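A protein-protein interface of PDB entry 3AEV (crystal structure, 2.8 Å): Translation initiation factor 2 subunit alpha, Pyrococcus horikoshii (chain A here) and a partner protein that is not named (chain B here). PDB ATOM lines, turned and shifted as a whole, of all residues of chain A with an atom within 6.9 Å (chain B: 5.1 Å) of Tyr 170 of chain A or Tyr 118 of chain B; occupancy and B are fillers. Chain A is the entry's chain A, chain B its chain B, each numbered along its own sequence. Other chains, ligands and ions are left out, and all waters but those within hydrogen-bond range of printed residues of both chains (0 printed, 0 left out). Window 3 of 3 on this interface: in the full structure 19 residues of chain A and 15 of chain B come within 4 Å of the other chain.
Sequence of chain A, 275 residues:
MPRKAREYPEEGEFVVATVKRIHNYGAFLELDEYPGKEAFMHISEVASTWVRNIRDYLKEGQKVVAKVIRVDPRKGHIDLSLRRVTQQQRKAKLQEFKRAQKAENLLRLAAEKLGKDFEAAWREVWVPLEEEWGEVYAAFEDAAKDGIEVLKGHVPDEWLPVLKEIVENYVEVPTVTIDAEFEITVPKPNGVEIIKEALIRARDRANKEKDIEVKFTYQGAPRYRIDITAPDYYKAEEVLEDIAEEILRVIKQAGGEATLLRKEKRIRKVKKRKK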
ATOM      1  N   LYS A 102       4.981  11.093  14.318  1.00  0.00           N
ATOM      2  CA  LYS A 102       5.300  10.342  15.529  1.00  0.00           C
ATOM      3  C   LYS A 102       6.238   9.190  15.188  1.00  0.00           C
ATOM      4  O   LYS A 102       7.260   8.957  15.851  1.00  0.00           O
ATOM      5  CB  LYS A 102       4.041   9.776  16.166  1.00  0.00           C
ATOM      6  CG  LYS A 102       3.453  10.651  17.259  1.00  0.00           C
ATOM      7  CD  LYS A 102       2.438   9.889  18.167  1.00  0.00           C
ATOM      8  CE  LYS A 102       0.952  10.149  17.789  1.00  0.00           C
ATOM      9  NZ  LYS A 102       0.052  10.032  18.984  1.00  0.00           N
ATOM     10  N   LEU A 106       9.879   8.630  16.783  1.00  0.00           N
ATOM     11  CA  LEU A 106      10.175   7.421  17.501  1.00  0.00           C
ATOM     12  C   LEU A 106      11.391   6.761  16.878  1.00  0.00           C
ATOM     13  O   LEU A 106      12.316   6.340  17.581  1.00  0.00           O
ATOM     14  CB  LEU A 106       8.980   6.520  17.460  1.00  0.00           C
ATOM     15  CG  LEU A 106       8.112   6.506  18.708  1.00  0.00           C
ATOM     16  CD1 LEU A 106       8.301   7.705  19.605  1.00  0.00           C
ATOM     17  CD2 LEU A 106       6.656   6.306  18.309  1.00  0.00           C
ATOM     18  N   LEU A 109      14.642   8.578  17.677  1.00  0.00           N
ATOM     19  CA  LEU A 109      15.061   8.297  19.014  1.00  0.00           C
ATOM     20  C   LEU A 109      15.759   6.930  19.087  1.00  0.00           C
ATOM     21  O   LEU A 109      16.823   6.795  19.716  1.00  0.00           O
ATOM     22  CB  LEU A 109      13.854   8.380  19.928  1.00  0.00           C
ATOM     23  CG  LEU A 109      14.011   8.091  21.416  1.00  0.00           C
ATOM     24  CD1 LEU A 109      15.175   8.857  22.094  1.00  0.00           C
ATOM     25  CD2 LEU A 109      12.665   8.370  22.080  1.00  0.00           C
ATOM     26  N   LYS A 113      19.693   6.154  20.168  1.00  0.00           N
ATOM     27  CA  LYS A 113      20.009   5.156  21.206  1.00  0.00           C
ATOM     28  C   LYS A 113      20.985   4.076  20.764  1.00  0.00           C
ATOM     29  O   LYS A 113      21.682   3.494  21.588  1.00  0.00           O
ATOM     30  CB  LYS A 113      18.760   4.459  21.734  1.00  0.00           C
ATOM     31  CG  LYS A 113      18.016   5.205  22.812  1.00  0.00           C
ATOM     32  CD  LYS A 113      16.790   4.422  23.207  1.00  0.00           C
ATOM     33  CE  LYS A 113      15.993   5.116  24.279  1.00  0.00           C
ATOM     34  NZ  LYS A 113      16.661   5.076  25.629  1.00  0.00           N
ATOM     35  N   TYR A 137       3.608   3.851  11.372  1.00  0.00           N
ATOM     36  CA  TYR A 137       2.936   3.848  12.685  1.00  0.00           C
ATOM     37  C   TYR A 137       2.141   2.555  12.907  1.00  0.00           C
ATOM     38  O   TYR A 137       2.047   2.068  14.032  1.00  0.00           O
ATOM     39  CB  TYR A 137       2.060   5.078  12.938  1.00  0.00           C
ATOM     40  CG  TYR A 137       1.857   5.373  14.426  1.00  0.00           C
ATOM     41  CD1 TYR A 137       2.874   5.961  15.200  1.00  0.00           C
ATOM     42  CD2 TYR A 137       0.648   5.051  15.067  1.00  0.00           C
ATOM     43  CE1 TYR A 137       2.689   6.225  16.574  1.00  0.00           C
ATOM     44  CE2 TYR A 137       0.450   5.309  16.428  1.00  0.00           C
ATOM     45  CZ  TYR A 137       1.476   5.887  17.195  1.00  0.00           C
ATOM     46  OH  TYR A 137       1.265   6.128  18.568  1.00  0.00           O
ATOM     47  N   VAL A 162      15.574  -2.047  20.992  1.00  0.00           N
ATOM     48  CA  VAL A 162      15.409  -0.647  21.285  1.00  0.00           C
ATOM     49  C   VAL A 162      14.092  -0.174  20.726  1.00  0.00           C
ATOM     50  O   VAL A 162      13.357   0.578  21.409  1.00  0.00           O
ATOM     51  CB  VAL A 162      16.629   0.214  20.855  1.00  0.00           C
ATOM     52  CG1 VAL A 162      17.325  -0.370  19.660  1.00  0.00           C
ATOM     53  CG2 VAL A 162      16.236   1.649  20.607  1.00  0.00           C
ATOM     54  N   GLU A 165      11.571  -1.109  23.417  1.00  0.00           N
ATOM     55  CA  GLU A 165      11.456  -0.202  24.539  1.00  0.00           C
ATOM     56  C   GLU A 165      10.630   1.039  24.135  1.00  0.00           C
ATOM     57  O   GLU A 165       9.687   1.440  24.834  1.00  0.00           O
ATOM     58  CB  GLU A 165      12.862   0.148  25.036  1.00  0.00           C
ATOM     59  CG  GLU A 165      12.931   1.327  25.949  1.00  0.00           C
ATOM     60  CD  GLU A 165      14.345   1.626  26.436  1.00  0.00           C
ATOM     61  OE1 GLU A 165      15.144   0.672  26.663  1.00  0.00           O
ATOM     62  OE2 GLU A 165      14.649   2.833  26.611  1.00  0.00           O
ATOM     63  N   ILE A 166      10.951   1.617  22.988  1.00  0.00           N
ATOM     64  CA  ILE A 166      10.253   2.795  22.516  1.00  0.00           C
ATOM     65  C   ILE A 166       8.784   2.544  22.175  1.00  0.00           C
ATOM     66  O   ILE A 166       7.908   3.320  22.615  1.00  0.00           O
ATOM     67  CB  ILE A 166      10.986   3.402  21.334  1.00  0.00           C
ATOM     68  CG1 ILE A 166      12.304   3.972  21.837  1.00  0.00           C
ATOM     69  CG2 ILE A 166      10.172   4.487  20.657  1.00  0.00           C
ATOM     70  CD1 ILE A 166      13.274   4.100  20.756  1.00  0.00           C
ATOM     71  N   VAL A 167       8.472   1.489  21.419  1.00  0.00           N
ATOM     72  CA  VAL A 167       7.066   1.353  21.073  1.00  0.00           C
ATOM     73  C   VAL A 167       6.261   1.035  22.299  1.00  0.00           C
ATOM     74  O   VAL A 167       5.213   1.649  22.516  1.00  0.00           O
ATOM     75  CB  VAL A 167       6.724   0.431  19.865  1.00  0.00           C
ATOM     76  CG1 VAL A 167       7.882   0.296  18.918  1.00  0.00           C
ATOM     77  CG2 VAL A 167       6.194  -0.915  20.289  1.00  0.00           C
ATOM     78  N   GLU A 168       6.750   0.124  23.133  1.00  0.00           N
ATOM     79  CA  GLU A 168       5.991  -0.215  24.332  1.00  0.00           C
ATOM     80  C   GLU A 168       5.681   0.996  25.203  1.00  0.00           C
ATOM     81  O   GLU A 168       4.670   1.009  25.885  1.00  0.00           O
ATOM     82  CB  GLU A 168       6.666  -1.309  25.141  1.00  0.00           C
ATOM     83  CG  GLU A 168       6.500  -2.640  24.477  1.00  0.00           C
ATOM     84  CD  GLU A 168       6.930  -3.800  25.343  1.00  0.00           C
ATOM     85  OE1 GLU A 168       6.337  -4.901  25.192  1.00  0.00           O
ATOM     86  OE2 GLU A 168       7.866  -3.615  26.166  1.00  0.00           O
ATOM     87  N   ASN A 169       6.517   2.025  25.186  1.00  0.00           N
ATOM     88  CA  ASN A 169       6.238   3.080  26.110  1.00  0.00           C
ATOM     89  C   ASN A 169       5.459   4.197  25.496  1.00  0.00           C
ATOM     90  O   ASN A 169       4.881   5.009  26.212  1.00  0.00           O
ATOM     91  CB  ASN A 169       7.489   3.529  26.872  1.00  0.00           C
ATOM     92  CG  ASN A 169       7.949   2.459  27.936  1.00  0.00           C
ATOM     93  OD1 ASN A 169       7.295   2.271  28.965  1.00  0.00           O
ATOM     94  ND2 ASN A 169       9.068   1.767  27.661  1.00  0.00           N
ATOM     95  N   TYR A 170       5.387   4.217  24.175  1.00  0.00           N
ATOM     96  CA  TYR A 170       4.863   5.409  23.463  1.00  0.00           C
ATOM     97  C   TYR A 170       3.704   5.156  22.487  1.00  0.00           C
ATOM     98  O   TYR A 170       3.012   6.099  22.092  1.00  0.00           O
ATOM     99  CB  TYR A 170       5.991   6.166  22.734  1.00  0.00           C
ATOM    100  CG  TYR A 170       6.990   6.867  23.651  1.00  0.00           C
ATOM    101  CD1 TYR A 170       8.264   6.327  23.888  1.00  0.00           C
ATOM    102  CD2 TYR A 170       6.669   8.080  24.268  1.00  0.00           C
ATOM    103  CE1 TYR A 170       9.181   6.979  24.726  1.00  0.00           C
ATOM    104  CE2 TYR A 170       7.574   8.730  25.099  1.00  0.00           C
ATOM    105  CZ  TYR A 170       8.826   8.180  25.329  1.00  0.00           C
ATOM    106  OH  TYR A 170       9.712   8.844  26.163  1.00  0.00           O
ATOM    107  N   VAL A 171       3.495   3.912  22.075  1.00  0.00           N
ATOM    108  CA  VAL A 171       2.369   3.680  21.234  1.00  0.00           C
ATOM    109  C   VAL A 171       1.320   2.795  21.867  1.00  0.00           C
ATOM    110  O   VAL A 171       1.584   1.647  22.193  1.00  0.00           O
ATOM    111  CB  VAL A 171       2.735   3.283  19.752  1.00  0.00           C
ATOM    112  CG1 VAL A 171       4.223   3.300  19.479  1.00  0.00           C
ATOM    113  CG2 VAL A 171       2.078   2.003  19.344  1.00  0.00           C
ATOM    114  N   GLU A 172       0.135   3.369  22.051  1.00  0.00           N
ATOM    115  CA  GLU A 172      -1.028   2.658  22.555  1.00  0.00           C
ATOM    116  C   GLU A 172      -1.523   1.526  21.651  1.00  0.00           C
ATOM    117  O   GLU A 172      -1.365   1.578  20.440  1.00  0.00           O
ATOM    118  CB  GLU A 172      -2.132   3.670  22.812  1.00  0.00           C
ATOM    119  CG  GLU A 172      -1.835   4.489  24.046  1.00  0.00           C
ATOM    120  CD  GLU A 172      -3.023   5.308  24.515  1.00  0.00           C
ATOM    121  OE1 GLU A 172      -2.793   6.318  25.228  1.00  0.00           O
ATOM    122  OE2 GLU A 172      -4.193   4.964  24.175  1.00  0.00           O
ATOM    123  N   LEU B  88       9.337  14.453  21.647  1.00  0.00           N
ATOM    124  CA  LEU B  88       8.644  13.552  22.577  1.00  0.00           C
ATOM    125  C   LEU B  88       8.048  14.261  23.786  1.00  0.00           C
ATOM    126  O   LEU B  88       7.388  13.645  24.608  1.00  0.00           O
ATOM    127  CB  LEU B  88       9.577  12.423  23.037  1.00  0.00           C
ATOM    128  CG  LEU B  88       9.720  11.220  22.098  1.00  0.00           C
ATOM    129  CD1 LEU B  88       8.368  10.877  21.482  1.00  0.00           C
ATOM    130  CD2 LEU B  88      10.736  11.475  21.009  1.00  0.00           C
ATOM    131  N   TRP B  91       4.486  13.649  25.237  1.00  0.00           N
ATOM    132  CA  TRP B  91       4.375  12.394  25.951  1.00  0.00           C
ATOM    133  C   TRP B  91       5.024  12.420  27.341  1.00  0.00           C
ATOM    134  O   TRP B  91       4.448  11.920  28.312  1.00  0.00           O
ATOM    135  CB  TRP B  91       4.879  11.264  25.069  1.00  0.00           C
ATOM    136  CG  TRP B  91       3.992  11.170  23.871  1.00  0.00           C
ATOM    137  CD1 TRP B  91       2.882  10.396  23.747  1.00  0.00           C
ATOM    138  CD2 TRP B  91       4.084  11.950  22.659  1.00  0.00           C
ATOM    139  NE1 TRP B  91       2.284  10.633  22.537  1.00  0.00           N
ATOM    140  CE2 TRP B  91       2.999  11.574  21.845  1.00  0.00           C
ATOM    141  CE3 TRP B  91       4.975  12.940  22.192  1.00  0.00           C
ATOM    142  CZ2 TRP B  91       2.770  12.136  20.573  1.00  0.00           C
ATOM    143  CZ3 TRP B  91       4.750  13.497  20.911  1.00  0.00           C
ATOM    144  CH2 TRP B  91       3.654  13.079  20.118  1.00  0.00           C
ATOM    145  N   LYS B  92       6.191  13.036  27.455  1.00  0.00           N
ATOM    146  CA  LYS B  92       6.790  13.216  28.762  1.00  0.00           C
ATOM    147  C   LYS B  92       5.876  14.016  29.688  1.00  0.00           C
ATOM    148  O   LYS B  92       5.675  13.643  30.853  1.00  0.00           O
ATOM    149  CB  LYS B  92       8.153  13.868  28.633  1.00  0.00           C
ATOM    150  CG  LYS B  92       9.180  12.966  27.977  1.00  0.00           C
ATOM    151  CD  LYS B  92      10.331  13.778  27.425  1.00  0.00           C
ATOM    152  CE  LYS B  92      11.592  12.927  27.284  1.00  0.00           C
ATOM    153  NZ  LYS B  92      12.778  13.757  26.871  1.00  0.00           N
ATOM    154  N   ASP B  95       3.088  12.011  30.926  1.00  0.00           N
ATOM    155  CA  ASP B  95       3.453  11.015  31.892  1.00  0.00           C
ATOM    156  C   ASP B  95       3.652  11.626  33.279  1.00  0.00           C
ATOM    157  O   ASP B  95       3.247  11.050  34.289  1.00  0.00           O
ATOM    158  CB  ASP B  95       4.631  10.215  31.379  1.00  0.00           C
ATOM    159  CG  ASP B  95       4.216   9.267  30.200  1.00  0.00           C
ATOM    160  OD1 ASP B  95       5.098   8.782  29.418  1.00  0.00           O
ATOM    161  OD2 ASP B  95       2.986   9.006  30.056  1.00  0.00           O
ATOM    162  N   LEU B 112      10.785  11.767  35.332  1.00  0.00           N
ATOM    163  CA  LEU B 112      10.384  11.305  34.023  1.00  0.00           C
ATOM    164  C   LEU B 112      10.951  12.138  32.877  1.00  0.00           C
ATOM    165  O   LEU B 112      10.792  11.762  31.693  1.00  0.00           O
ATOM    166  CB  LEU B 112       8.862  11.244  33.919  1.00  0.00           C
ATOM    167  CG  LEU B 112       8.193  10.085  34.654  1.00  0.00           C
ATOM    168  CD1 LEU B 112       6.757  10.388  34.961  1.00  0.00           C
ATOM    169  CD2 LEU B 112       8.279   8.804  33.880  1.00  0.00           C
ATOM    170  N   GLY B 116      15.289   7.958  28.977  1.00  0.00           N
ATOM    171  CA  GLY B 116      15.087   6.525  29.122  1.00  0.00           C
ATOM    172  C   GLY B 116      14.481   6.141  30.450  1.00  0.00           C
ATOM    173  O   GLY B 116      14.784   5.096  30.991  1.00  0.00           O
ATOM    174  N   GLU B 117      13.620   6.987  30.980  1.00  0.00           N
ATOM    175  CA  GLU B 117      12.903   6.635  32.183  1.00  0.00           C
ATOM    176  C   GLU B 117      11.423   6.759  31.921  1.00  0.00           C
ATOM    177  O   GLU B 117      10.974   7.727  31.322  1.00  0.00           O
ATOM    178  CB  GLU B 117      13.395   7.441  33.405  1.00  0.00           C
ATOM    179  CG  GLU B 117      14.924   7.313  33.548  1.00  0.00           C
ATOM    180  CD  GLU B 117      15.438   7.184  34.967  1.00  0.00           C
ATOM    181  OE1 GLU B 117      15.069   8.034  35.802  1.00  0.00           O
ATOM    182  OE2 GLU B 117      16.264   6.258  35.232  1.00  0.00           O
ATOM    183  N   TYR B 118      10.678   5.753  32.362  1.00  0.00           N
ATOM    184  CA  TYR B 118       9.329   5.537  31.933  1.00  0.00           C
ATOM    185  C   TYR B 118       8.492   5.355  33.165  1.00  0.00           C
ATOM    186  O   TYR B 118       9.009   5.032  34.230  1.00  0.00           O
ATOM    187  CB  TYR B 118       9.277   4.288  31.057  1.00  0.00           C
ATOM    188  CG  TYR B 118      10.205   4.377  29.881  1.00  0.00           C
ATOM    189  CD1 TYR B 118      10.109   5.436  28.976  1.00  0.00           C
ATOM    190  CD2 TYR B 118      11.206   3.436  29.691  1.00  0.00           C
ATOM    191  CE1 TYR B 118      10.967   5.530  27.912  1.00  0.00           C
ATOM    192  CE2 TYR B 118      12.087   3.529  28.612  1.00  0.00           C
ATOM    193  CZ  TYR B 118      11.952   4.569  27.725  1.00  0.00           C
ATOM    194  OH  TYR B 118      12.802   4.672  26.649  1.00  0.00           O
ATOM    195  N   LEU B 119       7.199   5.596  33.014  1.00  0.00           N
ATOM    196  CA  LEU B 119       6.223   5.413  34.057  1.00  0.00           C
ATOM    197  C   LEU B 119       5.432   4.168  33.752  1.00  0.00           C
ATOM    198  O   LEU B 119       5.019   3.961  32.626  1.00  0.00           O
ATOM    199  CB  LEU B 119       5.279   6.592  34.055  1.00  0.00           C
ATOM    200  CG  LEU B 119       4.000   6.378  34.830  1.00  0.00           C
ATOM    201  CD1 LEU B 119       4.270   6.485  36.346  1.00  0.00           C
ATOM    202  CD2 LEU B 119       3.030   7.405  34.403  1.00  0.00           C
ATOM    203  N   GLU B 120       5.209   3.353  34.764  1.00  0.00           N
ATOM    204  CA  GLU B 120       4.480   2.117  34.624  1.00  0.00           C
ATOM    205  C   GLU B 120       3.421   2.064  35.710  1.00  0.00           C
ATOM    206  O   GLU B 120       3.733   2.232  36.876  1.00  0.00           O
ATOM    207  CB  GLU B 120       5.427   0.945  34.767  1.00  0.00           C
ATOM    208  CG  GLU B 120       4.708  -0.352  35.078  1.00  0.00           C
ATOM    209  CD  GLU B 120       4.403  -1.211  33.839  1.00  0.00           C
ATOM    210  OE1 GLU B 120       3.426  -2.017  33.889  1.00  0.00           O
ATOM    211  OE2 GLU B 120       5.142  -1.099  32.833  1.00  0.00           O
ATOM    212  N   ILE B 171       5.314   3.041  39.188  1.00  0.00           N
ATOM    213  CA  ILE B 171       6.751   2.968  39.301  1.00  0.00           C
ATOM    214  C   ILE B 171       7.421   3.894  38.280  1.00  0.00           C
ATOM    215  O   ILE B 171       7.027   3.848  37.113  1.00  0.00           O
ATOM    216  CB  ILE B 171       7.152   1.552  38.931  1.00  0.00           C
ATOM    217  CG1 ILE B 171       6.454   0.536  39.833  1.00  0.00           C
ATOM    218  CG2 ILE B 171       8.627   1.379  38.989  1.00  0.00           C
ATOM    219  CD1 ILE B 171       6.478  -0.832  39.230  1.00  0.00           C
ATOM    220  N   ILE B 172       8.416   4.708  38.674  1.00  0.00           N
ATOM    221  CA  ILE B 172       9.242   5.424  37.695  1.00  0.00           C
ATOM    222  C   ILE B 172      10.634   4.795  37.657  1.00  0.00           C
ATOM    223  O   ILE B 172      11.228   4.570  38.716  1.00  0.00           O
ATOM    224  CB  ILE B 172       9.553   6.882  38.090  1.00  0.00           C
ATOM    225  CG1 ILE B 172       8.342   7.705  38.569  1.00  0.00           C
ATOM    226  CG2 ILE B 172      10.244   7.611  36.965  1.00  0.00           C
ATOM    227  CD1 ILE B 172       7.267   7.805  37.593  1.00  0.00           C
ATOM    228  N   GLY B 173      11.200   4.568  36.466  1.00  0.00           N
ATOM    229  CA  GLY B 173      12.594   4.105  36.358  1.00  0.00           C
ATOM    230  C   GLY B 173      12.944   3.709  34.939  1.00  0.00           C
ATOM    231  O   GLY B 173      12.137   3.907  34.040  1.00  0.00           O
ATOM    232  N   ASN B 174      14.140   3.165  34.705  1.00  0.00           N
ATOM    233  CA  ASN B 174      14.390   2.540  33.402  1.00  0.00           C
ATOM    234  C   ASN B 174      13.849   1.107  33.399  1.00  0.00           C
ATOM    235  O   ASN B 174      13.536   0.569  34.467  1.00  0.00           O
ATOM    236  CB  ASN B 174      15.871   2.583  33.018  1.00  0.00           C
ATOM    237  CG  ASN B 174      16.737   1.758  33.930  1.00  0.00           C
ATOM    238  OD1 ASN B 174      17.752   2.236  34.405  1.00  0.00           O
ATOM    239  ND2 ASN B 174      16.345   0.514  34.184  1.00  0.00           N
ATOM    240  N   PRO B 175      13.762   0.464  32.211  1.00  0.00           N
ATOM    241  CA  PRO B 175      13.019  -0.804  32.172  1.00  0.00           C
ATOM    242  C   PRO B 175      13.563  -1.861  33.130  1.00  0.00           C
ATOM    243  O   PRO B 175      12.765  -2.565  33.743  1.00  0.00           O
ATOM    244  CB  PRO B 175      13.154  -1.239  30.724  1.00  0.00           C
ATOM    245  CG  PRO B 175      13.379   0.050  29.994  1.00  0.00           C
ATOM    246  CD  PRO B 175      14.301   0.790  30.880  1.00  0.00           C
ATOM    247  N   ILE B 178      12.353  -0.869  36.535  1.00  0.00           N
ATOM    248  CA  ILE B 178      10.929  -1.134  36.584  1.00  0.00           C
ATOM    249  C   ILE B 178      10.633  -2.614  36.740  1.00  0.00           C
ATOM    250  O   ILE B 178       9.786  -2.999  37.553  1.00  0.00           O
ATOM    251  CB  ILE B 178      10.203  -0.546  35.385  1.00  0.00           C
ATOM    252  CG1 ILE B 178      10.189   0.991  35.519  1.00  0.00           C
ATOM    253  CG2 ILE B 178       8.761  -1.059  35.303  1.00  0.00           C
ATOM    254  CD1 ILE B 178       9.823   1.747  34.291  1.00  0.00           C
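Of the 16 printed residues of chain B, 4 touch a printed residue of chain A.
Printed residues of chain B that touch a printed residue of chain A: Leu 88, Trp 91, Tyr 118 and Pro 175.
Printed residues of chain A that touch a printed residue of chain B: Lys 102, Leu 106, Leu 109, Lys 113, Glu 165, Asn 169 and Tyr 170.
Along chain A the printed residues that touch a printed residue of chain B span positions 102 to 170.
Among the printed residues, 9 pairs touch across the chains.
Among the printed residues, no Asp or Glu carboxylate lies within 4 Å of a Lys or Arg side-chain nitrogen of the other chain.
Tyr 170 of chain A touches just these residues of chain B: Trp 91 and Tyr 118.
Of the printed residues of chain A, Tyr 118 of chain B touches Lys 113 (3.9996 Å), Glu 165 (2.6 Å), Asn 169 (3.4 Å) and Tyr 170 (3.9 Å).
Of the printed residues of chain A, Pro 175 of chain B touches Glu 165 (3.8 Å).
Of the printed residues of chain B, Asn 169 of chain A touches Tyr 118.
Ile 178 of chain B touches none of the printed residues of chain A.
Lys 92 of chain B touches none of the printed residues of chain A.
The nearest residue of chain B that does not touch Tyr 170 of chain A is Leu 88 of chain B (4.3 Å).
The nearest printed residue of chain A that does not touch Tyr 118 of chain B is Ile 166 of chain A (4.9 Å).
The side-chain hydroxyl (OH) of Tyr 118 of chain B is in hydrogen-bond range of the side-chain carboxylate (OE2) of Glu 165 of chain A, at 2.6 Å.
Among the printed residues, pairs that only touch across the chains: Lys 102 of chain A with Trp 91 of chain B (3.3 Å), Asn 169 of chain A with Tyr 118 of chain B (3.4 Å), Leu 106 of chain A with Leu 88 of chain B (3.7 Å), Tyr 170 of chain A with Trp 91 of chain B (3.7 Å), Leu 109 of chain A with Leu 88 of chain B (3.8 Å), Glu 165 of chain A with Pro 175 of chain B (3.8 Å), Tyr 170 of chain A with Tyr 118 of chain B (3.9 Å) and Lys 113 of chain A with Tyr 118 of chain B (3.9996 Å).
The side-chain amino group (NZ) of Lys 113 of chain A lies within salt-bridge range of the side-chain carboxylate (OE2) of Glu 165 of chain A, 3.2 Å away.
ND2 of Asn 169 of chain A lies within hydrogen-bond range of O of Glu 165 of chain A (2.9 Å).
The backbone NH of Tyr 118 of chain B is in hydrogen-bond range of the backbone carbonyl oxygen of Gly 173 of chain B (2.9 Å).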
